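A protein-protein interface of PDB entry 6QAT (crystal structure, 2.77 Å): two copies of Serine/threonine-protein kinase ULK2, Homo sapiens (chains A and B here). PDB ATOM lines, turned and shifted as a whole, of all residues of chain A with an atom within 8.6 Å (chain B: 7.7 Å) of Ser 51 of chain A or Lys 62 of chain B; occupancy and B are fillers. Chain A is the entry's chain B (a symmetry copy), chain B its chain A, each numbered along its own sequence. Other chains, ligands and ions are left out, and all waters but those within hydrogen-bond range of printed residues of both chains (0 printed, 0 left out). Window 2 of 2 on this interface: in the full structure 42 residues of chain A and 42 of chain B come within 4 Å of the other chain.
The side-chain amino group of Lys 62 of chain B sits at hydrogen-bond distance from the backbone carbonyl oxygen of Leu 50 of chain A, 3.5 Å away. NZ of Lys 62 of chain B sits at hydrogen-bond distance from O of Ser 53 of chain A (2.9 Å).
O of Ser 51 of chain A touches NZ of Lys 62 of chain B (3.7 Å). Gln 54 of chain A touches Tyr 168 of chain B (NE2 to CB, 3.3 Å). CE of Lys 62 of chain B touches O of Ile 55 of chain A (3.8 Å). Leu 56 of chain A touches Lys 59 of chain B (CD2 to CG, 3.7 Å). Leu 56 of chain A touches Lys 62 of chain B (CD2 to CD, 3.8 Å).
Of the 16 printed residues of chain B, 3 touch a printed residue of chain A. Of the 15 printed residues of chain A, 6 touch a printed residue of chain B. Hydrophobic or aromatic side chains of chain A within 4 Å of the printed part of chain B: Leu 56. Among the printed residues, no Asp or Glu carboxylate lies within 4 Å of a Lys or Arg side-chain nitrogen of the other chain.
Ser 51 of chain A touches just one residue of chain B: Lys 62. Of the printed residues of chain A, Lys 62 of chain B touches Leu 50 (3.5 Å), Ser 51 (3.7 Å), Ser 53 (2.9 Å), Ile 55 (3.8 Å) and Leu 56 (3.8 Å). Printed residues of chain B within 4 Å of Ile 55 of chain A: Lys 62. Of the printed residues of chain B, Ser 53 of chain A touches Lys 62 (2.9 Å). Of the printed residues of chain A, Tyr 168 of chain B touches Gln 54 (3.3 Å). Printed residues of chain B within 4 Å of Leu 50 of chain A: Lys 62 (3.5 Å). Leu 75 of chain B touches none of the printed residues of chain A. The nearest residue of chain A that does not touch Lys 62 of chain B is Gln 54 of chain A (4.05 Å).
3 positions are printed for both chains.
The side-chain carboxylate (OE2) of Glu 66 of chain B sits at hydrogen-bond distance from the side-chain hydroxyl (OH) of Tyr 168 of chain B. The backbone carbonyl oxygen (O) of Lys 48 of chain A sits at hydrogen-bond distance from the side-chain hydroxyl (OG) of Ser 51 of chain A (3.1 Å). O of Leu 50 of chain A lies within hydrogen-bond range of OG of Ser 53 of chain A, at 2.7 Å. N of Ile 55 of chain A sits at hydrogen-bond distance from OG of Ser 53 of chain A (3.1 Å).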
ATOM      1  N   PHE A  24       0.747  -7.554  24.494  1.00  0.00           N
ATOM      2  CA  PHE A  24      -0.173  -6.752  25.336  1.00  0.00           C
ATOM      3  C   PHE A  24      -1.487  -6.517  24.567  1.00  0.00           C
ATOM      4  O   PHE A  24      -2.286  -5.655  24.990  1.00  0.00           O
ATOM      5  CB  PHE A  24       0.487  -5.430  25.734  1.00  0.00           C
ATOM      6  CG  PHE A  24       1.928  -5.539  26.164  1.00  0.00           C
ATOM      7  CD1 PHE A  24       2.272  -6.011  27.434  1.00  0.00           C
ATOM      8  CD2 PHE A  24       2.947  -5.160  25.302  1.00  0.00           C
ATOM      9  CE1 PHE A  24       3.599  -6.082  27.827  1.00  0.00           C
ATOM     10  CE2 PHE A  24       4.274  -5.223  25.705  1.00  0.00           C
ATOM     11  CZ  PHE A  24       4.596  -5.683  26.965  1.00  0.00           C
ATOM     12  N   ILE A  45      -5.133  -3.039  22.503  1.00  0.00           N
ATOM     13  CA  ILE A  45      -3.780  -2.943  23.121  1.00  0.00           C
ATOM     14  C   ILE A  45      -3.908  -2.244  24.466  1.00  0.00           C
ATOM     15  O   ILE A  45      -4.370  -1.113  24.489  1.00  0.00           O
ATOM     16  CB  ILE A  45      -2.797  -2.205  22.204  1.00  0.00           C
ATOM     17  CG1 ILE A  45      -2.820  -2.748  20.783  1.00  0.00           C
ATOM     18  CG2 ILE A  45      -1.391  -2.236  22.792  1.00  0.00           C
ATOM     19  CD1 ILE A  45      -1.955  -1.932  19.808  1.00  0.00           C
ATOM     20  N   ASN A  46      -3.517  -2.925  25.537  1.00  0.00           N
ATOM     21  CA  ASN A  46      -3.514  -2.391  26.910  1.00  0.00           C
ATOM     22  C   ASN A  46      -2.470  -1.276  27.010  1.00  0.00           C
ATOM     23  O   ASN A  46      -1.265  -1.563  26.759  1.00  0.00           O
ATOM     24  CB  ASN A  46      -3.245  -3.505  27.912  1.00  0.00           C
ATOM     25  CG  ASN A  46      -3.412  -3.066  29.342  1.00  0.00           C
ATOM     26  OD1 ASN A  46      -2.731  -2.136  29.805  1.00  0.00           O
ATOM     27  ND2 ASN A  46      -4.123  -3.876  30.108  1.00  0.00           N
ATOM     28  N   LYS A  47      -2.906  -0.060  27.356  1.00  0.00           N
ATOM     29  CA  LYS A  47      -2.063   1.161  27.368  1.00  0.00           C
ATOM     30  C   LYS A  47      -1.024   1.062  28.497  1.00  0.00           C
ATOM     31  O   LYS A  47       0.158   1.366  28.235  1.00  0.00           O
ATOM     32  CB  LYS A  47      -2.927   2.420  27.532  1.00  0.00           C
ATOM     33  CG  LYS A  47      -3.642   2.883  26.281  1.00  0.00           C
ATOM     34  CD  LYS A  47      -4.754   3.866  26.552  1.00  0.00           C
ATOM     35  CE  LYS A  47      -4.315   5.313  26.459  1.00  0.00           C
ATOM     36  NZ  LYS A  47      -5.406   6.244  26.851  1.00  0.00           N
ATOM     37  N   LYS A  48      -1.457   0.695  29.708  1.00  0.00           N
ATOM     38  CA  LYS A  48      -0.574   0.603  30.903  1.00  0.00           C
ATOM     39  C   LYS A  48       0.563  -0.382  30.606  1.00  0.00           C
ATOM     40  O   LYS A  48       1.730  -0.052  30.922  1.00  0.00           O
ATOM     41  CB  LYS A  48      -1.359   0.173  32.158  1.00  0.00           C
ATOM     42  CG  LYS A  48      -2.004   1.314  32.950  1.00  0.00           C
ATOM     43  CD  LYS A  48      -1.745   1.263  34.457  1.00  0.00           C
ATOM     44  CE  LYS A  48      -1.864   2.626  35.110  1.00  0.00           C
ATOM     45  NZ  LYS A  48      -1.972   2.523  36.584  1.00  0.00           N
ATOM     46  N   ASN A  49       0.231  -1.535  30.003  1.00  0.00           N
ATOM     47  CA  ASN A  49       1.202  -2.577  29.587  1.00  0.00           C
ATOM     48  C   ASN A  49       2.186  -1.966  28.594  1.00  0.00           C
ATOM     49  O   ASN A  49       3.408  -2.106  28.816  1.00  0.00           O
ATOM     50  CB  ASN A  49       0.510  -3.785  28.958  1.00  0.00           C
ATOM     51  CG  ASN A  49       0.128  -4.848  29.963  1.00  0.00           C
ATOM     52  OD1 ASN A  49       0.713  -4.929  31.035  1.00  0.00           O
ATOM     53  ND2 ASN A  49      -0.837  -5.686  29.609  1.00  0.00           N
ATOM     54  N   LEU A  50       1.662  -1.331  27.539  1.00  0.00           N
ATOM     55  CA  LEU A  50       2.454  -0.684  26.477  1.00  0.00           C
ATOM     56  C   LEU A  50       3.420   0.330  27.105  1.00  0.00           C
ATOM     57  O   LEU A  50       4.617   0.305  26.740  1.00  0.00           O
ATOM     58  CB  LEU A  50       1.505  -0.008  25.484  1.00  0.00           C
ATOM     59  CG  LEU A  50       2.157   0.475  24.188  1.00  0.00           C
ATOM     60  CD1 LEU A  50       2.614  -0.702  23.342  1.00  0.00           C
ATOM     61  CD2 LEU A  50       1.212   1.367  23.401  1.00  0.00           C
ATOM     62  N   SER A  51       2.925   1.183  28.010  1.00  0.00           N
ATOM     63  CA  SER A  51       3.672   2.341  28.576  1.00  0.00           C
ATOM     64  C   SER A  51       4.869   1.844  29.394  1.00  0.00           C
ATOM     65  O   SER A  51       5.765   2.633  29.636  1.00  0.00           O
ATOM     66  CB  SER A  51       2.777   3.229  29.401  1.00  0.00           C
ATOM     67  OG  SER A  51       2.794   2.834  30.770  1.00  0.00           O
ATOM     68  N   LYS A  52       4.846   0.580  29.813  1.00  0.00           N
ATOM     69  CA  LYS A  52       5.919  -0.066  30.622  1.00  0.00           C
ATOM     70  C   LYS A  52       6.839  -0.878  29.692  1.00  0.00           C
ATOM     71  O   LYS A  52       7.867  -1.359  30.163  1.00  0.00           O
ATOM     72  CB  LYS A  52       5.297  -0.958  31.704  1.00  0.00           C
ATOM     73  CG  LYS A  52       4.488  -0.225  32.762  1.00  0.00           C
ATOM     74  CD  LYS A  52       3.933  -1.164  33.850  1.00  0.00           C
ATOM     75  CE  LYS A  52       3.062  -0.456  34.869  1.00  0.00           C
ATOM     76  NZ  LYS A  52       3.190  -1.061  36.223  1.00  0.00           N
ATOM     77  N   SER A  53       6.445  -1.035  28.427  1.00  0.00           N
ATOM     78  CA  SER A  53       7.219  -1.723  27.364  1.00  0.00           C
ATOM     79  C   SER A  53       8.058  -0.697  26.586  1.00  0.00           C
ATOM     80  O   SER A  53       7.968   0.520  26.904  1.00  0.00           O
ATOM     81  CB  SER A  53       6.310  -2.471  26.449  1.00  0.00           C
ATOM     82  OG  SER A  53       5.863  -1.631  25.390  1.00  0.00           O
ATOM     83  N   GLN A  54       8.828  -1.163  25.598  1.00  0.00           N
ATOM     84  CA  GLN A  54       9.655  -0.310  24.700  1.00  0.00           C
ATOM     85  C   GLN A  54       9.090  -0.394  23.282  1.00  0.00           C
ATOM     86  O   GLN A  54       9.788   0.043  22.341  1.00  0.00           O
ATOM     87  CB  GLN A  54      11.116  -0.744  24.751  1.00  0.00           C
ATOM     88  CG  GLN A  54      11.674  -0.798  26.159  1.00  0.00           C
ATOM     89  CD  GLN A  54      13.084  -1.324  26.166  1.00  0.00           C
ATOM     90  OE1 GLN A  54      13.378  -2.362  25.565  1.00  0.00           O
ATOM     91  NE2 GLN A  54      13.985  -0.571  26.787  1.00  0.00           N
ATOM     92  N   ILE A  55       7.866  -0.912  23.149  1.00  0.00           N
ATOM     93  CA  ILE A  55       7.095  -0.927  21.877  1.00  0.00           C
ATOM     94  C   ILE A  55       6.803   0.517  21.462  1.00  0.00           C
ATOM     95  O   ILE A  55       6.248   1.280  22.294  1.00  0.00           O
ATOM     96  CB  ILE A  55       5.803  -1.736  22.027  1.00  0.00           C
ATOM     97  CG1 ILE A  55       6.087  -3.186  22.404  1.00  0.00           C
ATOM     98  CG2 ILE A  55       4.957  -1.641  20.768  1.00  0.00           C
ATOM     99  CD1 ILE A  55       6.662  -4.008  21.269  1.00  0.00           C
ATOM    100  N   LEU A  56       7.115   0.858  20.218  1.00  0.00           N
ATOM    101  CA  LEU A  56       6.777   2.152  19.609  1.00  0.00           C
ATOM    102  C   LEU A  56       5.563   1.969  18.702  1.00  0.00           C
ATOM    103  O   LEU A  56       5.750   1.822  17.517  1.00  0.00           O
ATOM    104  CB  LEU A  56       7.996   2.672  18.846  1.00  0.00           C
ATOM    105  CG  LEU A  56       9.277   2.750  19.662  1.00  0.00           C
ATOM    106  CD1 LEU A  56      10.455   3.189  18.796  1.00  0.00           C
ATOM    107  CD2 LEU A  56       9.107   3.688  20.848  1.00  0.00           C
ATOM    108  N   LEU A  57       4.364   2.046  19.272  1.00  0.00           N
ATOM    109  CA  LEU A  57       3.073   1.907  18.545  1.00  0.00           C
ATOM    110  C   LEU A  57       2.912   3.066  17.565  1.00  0.00           C
ATOM    111  O   LEU A  57       2.389   2.834  16.492  1.00  0.00           O
ATOM    112  CB  LEU A  57       1.928   1.892  19.563  1.00  0.00           C
ATOM    113  CG  LEU A  57       0.544   1.590  19.000  1.00  0.00           C
ATOM    114  CD1 LEU A  57       0.551   0.317  18.192  1.00  0.00           C
ATOM    115  CD2 LEU A  57      -0.475   1.487  20.107  1.00  0.00           C
ATOM    116  N   GLY A  58       3.290   4.277  17.971  1.00  0.00           N
ATOM    117  CA  GLY A  58       3.299   5.470  17.108  1.00  0.00           C
ATOM    118  C   GLY A  58       4.034   5.203  15.811  1.00  0.00           C
ATOM    119  O   GLY A  58       3.488   5.513  14.756  1.00  0.00           O
ATOM    120  N   LEU B  56      10.082  10.052  14.385  1.00  0.00           N
ATOM    121  CA  LEU B  56       9.155   9.305  15.249  1.00  0.00           C
ATOM    122  C   LEU B  56       8.841  10.161  16.470  1.00  0.00           C
ATOM    123  O   LEU B  56       9.498   9.983  17.492  1.00  0.00           O
ATOM    124  CB  LEU B  56       9.808   7.983  15.639  1.00  0.00           C
ATOM    125  CG  LEU B  56      10.319   7.147  14.479  1.00  0.00           C
ATOM    126  CD1 LEU B  56      11.017   5.891  14.987  1.00  0.00           C
ATOM    127  CD2 LEU B  56       9.187   6.787  13.524  1.00  0.00           C
ATOM    128  N   LEU B  57       7.874  11.053  16.352  1.00  0.00           N
ATOM    129  CA  LEU B  57       7.500  12.017  17.413  1.00  0.00           C
ATOM    130  C   LEU B  57       6.934  11.263  18.617  1.00  0.00           C
ATOM    131  O   LEU B  57       7.200  11.679  19.746  1.00  0.00           O
ATOM    132  CB  LEU B  57       6.471  13.002  16.852  1.00  0.00           C
ATOM    133  CG  LEU B  57       6.115  14.157  17.767  1.00  0.00           C
ATOM    134  CD1 LEU B  57       7.373  14.874  18.231  1.00  0.00           C
ATOM    135  CD2 LEU B  57       5.159  15.110  17.077  1.00  0.00           C
ATOM    136  N   GLY B  58       6.102  10.263  18.362  1.00  0.00           N
ATOM    137  CA  GLY B  58       5.559   9.362  19.386  1.00  0.00           C
ATOM    138  C   GLY B  58       6.648   8.808  20.269  1.00  0.00           C
ATOM    139  O   GLY B  58       6.474   8.824  21.465  1.00  0.00           O
ATOM    140  N   LYS B  59       7.766   8.372  19.683  1.00  0.00           N
ATOM    141  CA  LYS B  59       8.913   7.811  20.425  1.00  0.00           C
ATOM    142  C   LYS B  59       9.485   8.896  21.332  1.00  0.00           C
ATOM    143  O   LYS B  59       9.742   8.612  22.530  1.00  0.00           O
ATOM    144  CB  LYS B  59       9.970   7.276  19.467  1.00  0.00           C
ATOM    145  CG  LYS B  59      11.203   6.718  20.154  1.00  0.00           C
ATOM    146  CD  LYS B  59      12.383   6.521  19.246  1.00  0.00           C
ATOM    147  CE  LYS B  59      13.051   7.810  18.836  1.00  0.00           C
ATOM    148  NZ  LYS B  59      14.092   7.561  17.805  1.00  0.00           N
ATOM    149  N   GLU B  60       9.691  10.085  20.797  1.00  0.00           N
ATOM    150  CA  GLU B  60      10.306  11.202  21.542  1.00  0.00           C
ATOM    151  C   GLU B  60       9.402  11.562  22.745  1.00  0.00           C
ATOM    152  O   GLU B  60       9.928  11.736  23.859  1.00  0.00           O
ATOM    153  CB  GLU B  60      10.561  12.381  20.623  1.00  0.00           C
ATOM    154  CG  GLU B  60      11.420  13.429  21.279  1.00  0.00           C
ATOM    155  CD  GLU B  60      11.751  14.641  20.445  1.00  0.00           C
ATOM    156  OE1 GLU B  60      11.501  14.596  19.178  1.00  0.00           O
ATOM    157  OE2 GLU B  60      12.310  15.638  21.052  1.00  0.00           O
ATOM    158  N   ILE B  61       8.098  11.577  22.546  1.00  0.00           N
ATOM    159  CA  ILE B  61       7.097  11.849  23.616  1.00  0.00           C
ATOM    160  C   ILE B  61       7.168  10.717  24.655  1.00  0.00           C
ATOM    161  O   ILE B  61       7.210  11.026  25.863  1.00  0.00           O
ATOM    162  CB  ILE B  61       5.681  12.005  23.024  1.00  0.00           C
ATOM    163  CG1 ILE B  61       5.584  13.222  22.101  1.00  0.00           C
ATOM    164  CG2 ILE B  61       4.638  12.056  24.128  1.00  0.00           C
ATOM    165  CD1 ILE B  61       4.380  13.215  21.206  1.00  0.00           C
ATOM    166  N   LYS B  62       7.235   9.471  24.194  1.00  0.00           N
ATOM    167  CA  LYS B  62       7.337   8.278  25.063  1.00  0.00           C
ATOM    168  C   LYS B  62       8.567   8.421  25.970  1.00  0.00           C
ATOM    169  O   LYS B  62       8.415   8.285  27.177  1.00  0.00           O
ATOM    170  CB  LYS B  62       7.388   7.004  24.228  1.00  0.00           C
ATOM    171  CG  LYS B  62       7.543   5.732  25.044  1.00  0.00           C
ATOM    172  CD  LYS B  62       7.565   4.480  24.253  1.00  0.00           C
ATOM    173  CE  LYS B  62       7.799   3.261  25.120  1.00  0.00           C
ATOM    174  NZ  LYS B  62       6.689   3.052  26.109  1.00  0.00           N
ATOM    175  N   ILE B  63       9.702   8.813  25.412  1.00  0.00           N
ATOM    176  CA  ILE B  63      10.997   8.895  26.151  1.00  0.00           C
ATOM    177  C   ILE B  63      10.956  10.088  27.100  1.00  0.00           C
ATOM    178  O   ILE B  63      11.364   9.934  28.248  1.00  0.00           O
ATOM    179  CB  ILE B  63      12.190   8.974  25.180  1.00  0.00           C
ATOM    180  CG1 ILE B  63      12.460   7.633  24.512  1.00  0.00           C
ATOM    181  CG2 ILE B  63      13.428   9.514  25.883  1.00  0.00           C
ATOM    182  CD1 ILE B  63      13.394   7.733  23.340  1.00  0.00           C
ATOM    183  N   LEU B  64      10.522  11.241  26.617  1.00  0.00           N
ATOM    184  CA  LEU B  64      10.420  12.479  27.437  1.00  0.00           C
ATOM    185  C   LEU B  64       9.510  12.228  28.653  1.00  0.00           C
ATOM    186  O   LEU B  64       9.820  12.744  29.716  1.00  0.00           O
ATOM    187  CB  LEU B  64       9.869  13.598  26.577  1.00  0.00           C
ATOM    188  CG  LEU B  64      10.875  14.327  25.709  1.00  0.00           C
ATOM    189  CD1 LEU B  64      10.155  15.334  24.828  1.00  0.00           C
ATOM    190  CD2 LEU B  64      11.942  15.010  26.543  1.00  0.00           C
ATOM    191  N   LYS B  65       8.402  11.496  28.463  1.00  0.00           N
ATOM    192  CA  LYS B  65       7.397  11.180  29.522  1.00  0.00           C
ATOM    193  C   LYS B  65       8.069  10.336  30.596  1.00  0.00           C
ATOM    194  O   LYS B  65       7.795  10.550  31.766  1.00  0.00           O
ATOM    195  CB  LYS B  65       6.191  10.440  28.930  1.00  0.00           C
ATOM    196  CG  LYS B  65       5.041  11.318  28.440  1.00  0.00           C
ATOM    197  CD  LYS B  65       3.882  10.490  27.816  1.00  0.00           C
ATOM    198  CE  LYS B  65       2.476  11.025  28.110  1.00  0.00           C
ATOM    199  NZ  LYS B  65       1.830  11.636  26.902  1.00  0.00           N
ATOM    200  N   GLU B  66       8.931   9.425  30.181  1.00  0.00           N
ATOM    201  CA  GLU B  66       9.600   8.422  31.042  1.00  0.00           C
ATOM    202  C   GLU B  66      10.700   9.114  31.891  1.00  0.00           C
ATOM    203  O   GLU B  66      11.012   8.620  32.953  1.00  0.00           O
ATOM    204  CB  GLU B  66      10.152   7.314  30.148  1.00  0.00           C
ATOM    205  CG  GLU B  66      10.724   6.154  30.904  1.00  0.00           C
ATOM    206  CD  GLU B  66      11.155   4.995  30.035  1.00  0.00           C
ATOM    207  OE1 GLU B  66      12.019   4.196  30.499  1.00  0.00           O
ATOM    208  OE2 GLU B  66      10.609   4.861  28.912  1.00  0.00           O
ATOM    209  N   LEU B  67      11.287  10.180  31.378  1.00  0.00           N
ATOM    210  CA  LEU B  67      12.404  10.938  32.019  1.00  0.00           C
ATOM    211  C   LEU B  67      11.839  12.143  32.764  1.00  0.00           C
ATOM    212  O   LEU B  67      11.330  13.035  32.119  1.00  0.00           O
ATOM    213  CB  LEU B  67      13.406  11.379  30.941  1.00  0.00           C
ATOM    214  CG  LEU B  67      14.011  10.238  30.137  1.00  0.00           C
ATOM    215  CD1 LEU B  67      14.767  10.750  28.923  1.00  0.00           C
ATOM    216  CD2 LEU B  67      14.925   9.401  31.009  1.00  0.00           C
ATOM    217  N   LEU B  75       8.777  17.781  29.495  1.00  0.00           N
ATOM    218  CA  LEU B  75       7.561  17.804  28.659  1.00  0.00           C
ATOM    219  C   LEU B  75       6.355  17.866  29.578  1.00  0.00           C
ATOM    220  O   LEU B  75       6.230  16.990  30.408  1.00  0.00           O
ATOM    221  CB  LEU B  75       7.506  16.541  27.793  1.00  0.00           C
ATOM    222  CG  LEU B  75       6.266  16.398  26.907  1.00  0.00           C
ATOM    223  CD1 LEU B  75       6.165  17.535  25.902  1.00  0.00           C
ATOM    224  CD2 LEU B  75       6.288  15.085  26.179  1.00  0.00           C
ATOM    225  N   VAL B  78       1.096  17.615  25.531  1.00  0.00           N
ATOM    226  CA  VAL B  78       1.011  17.453  24.063  1.00  0.00           C
ATOM    227  C   VAL B  78      -0.417  17.804  23.614  1.00  0.00           C
ATOM    228  O   VAL B  78      -1.368  17.179  24.129  1.00  0.00           O
ATOM    229  CB  VAL B  78       1.385  16.032  23.657  1.00  0.00           C
ATOM    230  CG1 VAL B  78       1.255  15.815  22.164  1.00  0.00           C
ATOM    231  CG2 VAL B  78       2.775  15.683  24.118  1.00  0.00           C
ATOM    232  N   ILE B 131      18.226   3.961  27.771  1.00  0.00           N
ATOM    233  CA  ILE B 131      18.038   4.906  26.627  1.00  0.00           C
ATOM    234  C   ILE B 131      19.395   5.413  26.169  1.00  0.00           C
ATOM    235  O   ILE B 131      20.088   6.015  26.983  1.00  0.00           O
ATOM    236  CB  ILE B 131      17.136   6.077  27.020  1.00  0.00           C
ATOM    237  CG1 ILE B 131      15.746   5.611  27.441  1.00  0.00           C
ATOM    238  CG2 ILE B 131      17.080   7.095  25.884  1.00  0.00           C
ATOM    239  CD1 ILE B 131      14.945   6.666  28.135  1.00  0.00           C
ATOM    240  N   TYR B 168      15.838   2.805  22.702  1.00  0.00           N
ATOM    241  CA  TYR B 168      15.867   1.890  23.855  1.00  0.00           C
ATOM    242  C   TYR B 168      16.799   0.734  23.545  1.00  0.00           C
ATOM    243  O   TYR B 168      16.718   0.214  22.440  1.00  0.00           O
ATOM    244  CB  TYR B 168      14.459   1.378  24.153  1.00  0.00           C
ATOM    245  CG  TYR B 168      13.529   2.390  24.760  1.00  0.00           C
ATOM    246  CD1 TYR B 168      13.568   2.671  26.116  1.00  0.00           C
ATOM    247  CD2 TYR B 168      12.592   3.052  23.990  1.00  0.00           C
ATOM    248  CE1 TYR B 168      12.722   3.604  26.682  1.00  0.00           C
ATOM    249  CE2 TYR B 168      11.699   3.954  24.554  1.00  0.00           C
ATOM    250  CZ  TYR B 168      11.765   4.223  25.908  1.00  0.00           C
ATOM    251  OH  TYR B 168      10.895   5.084  26.496  1.00  0.00           O
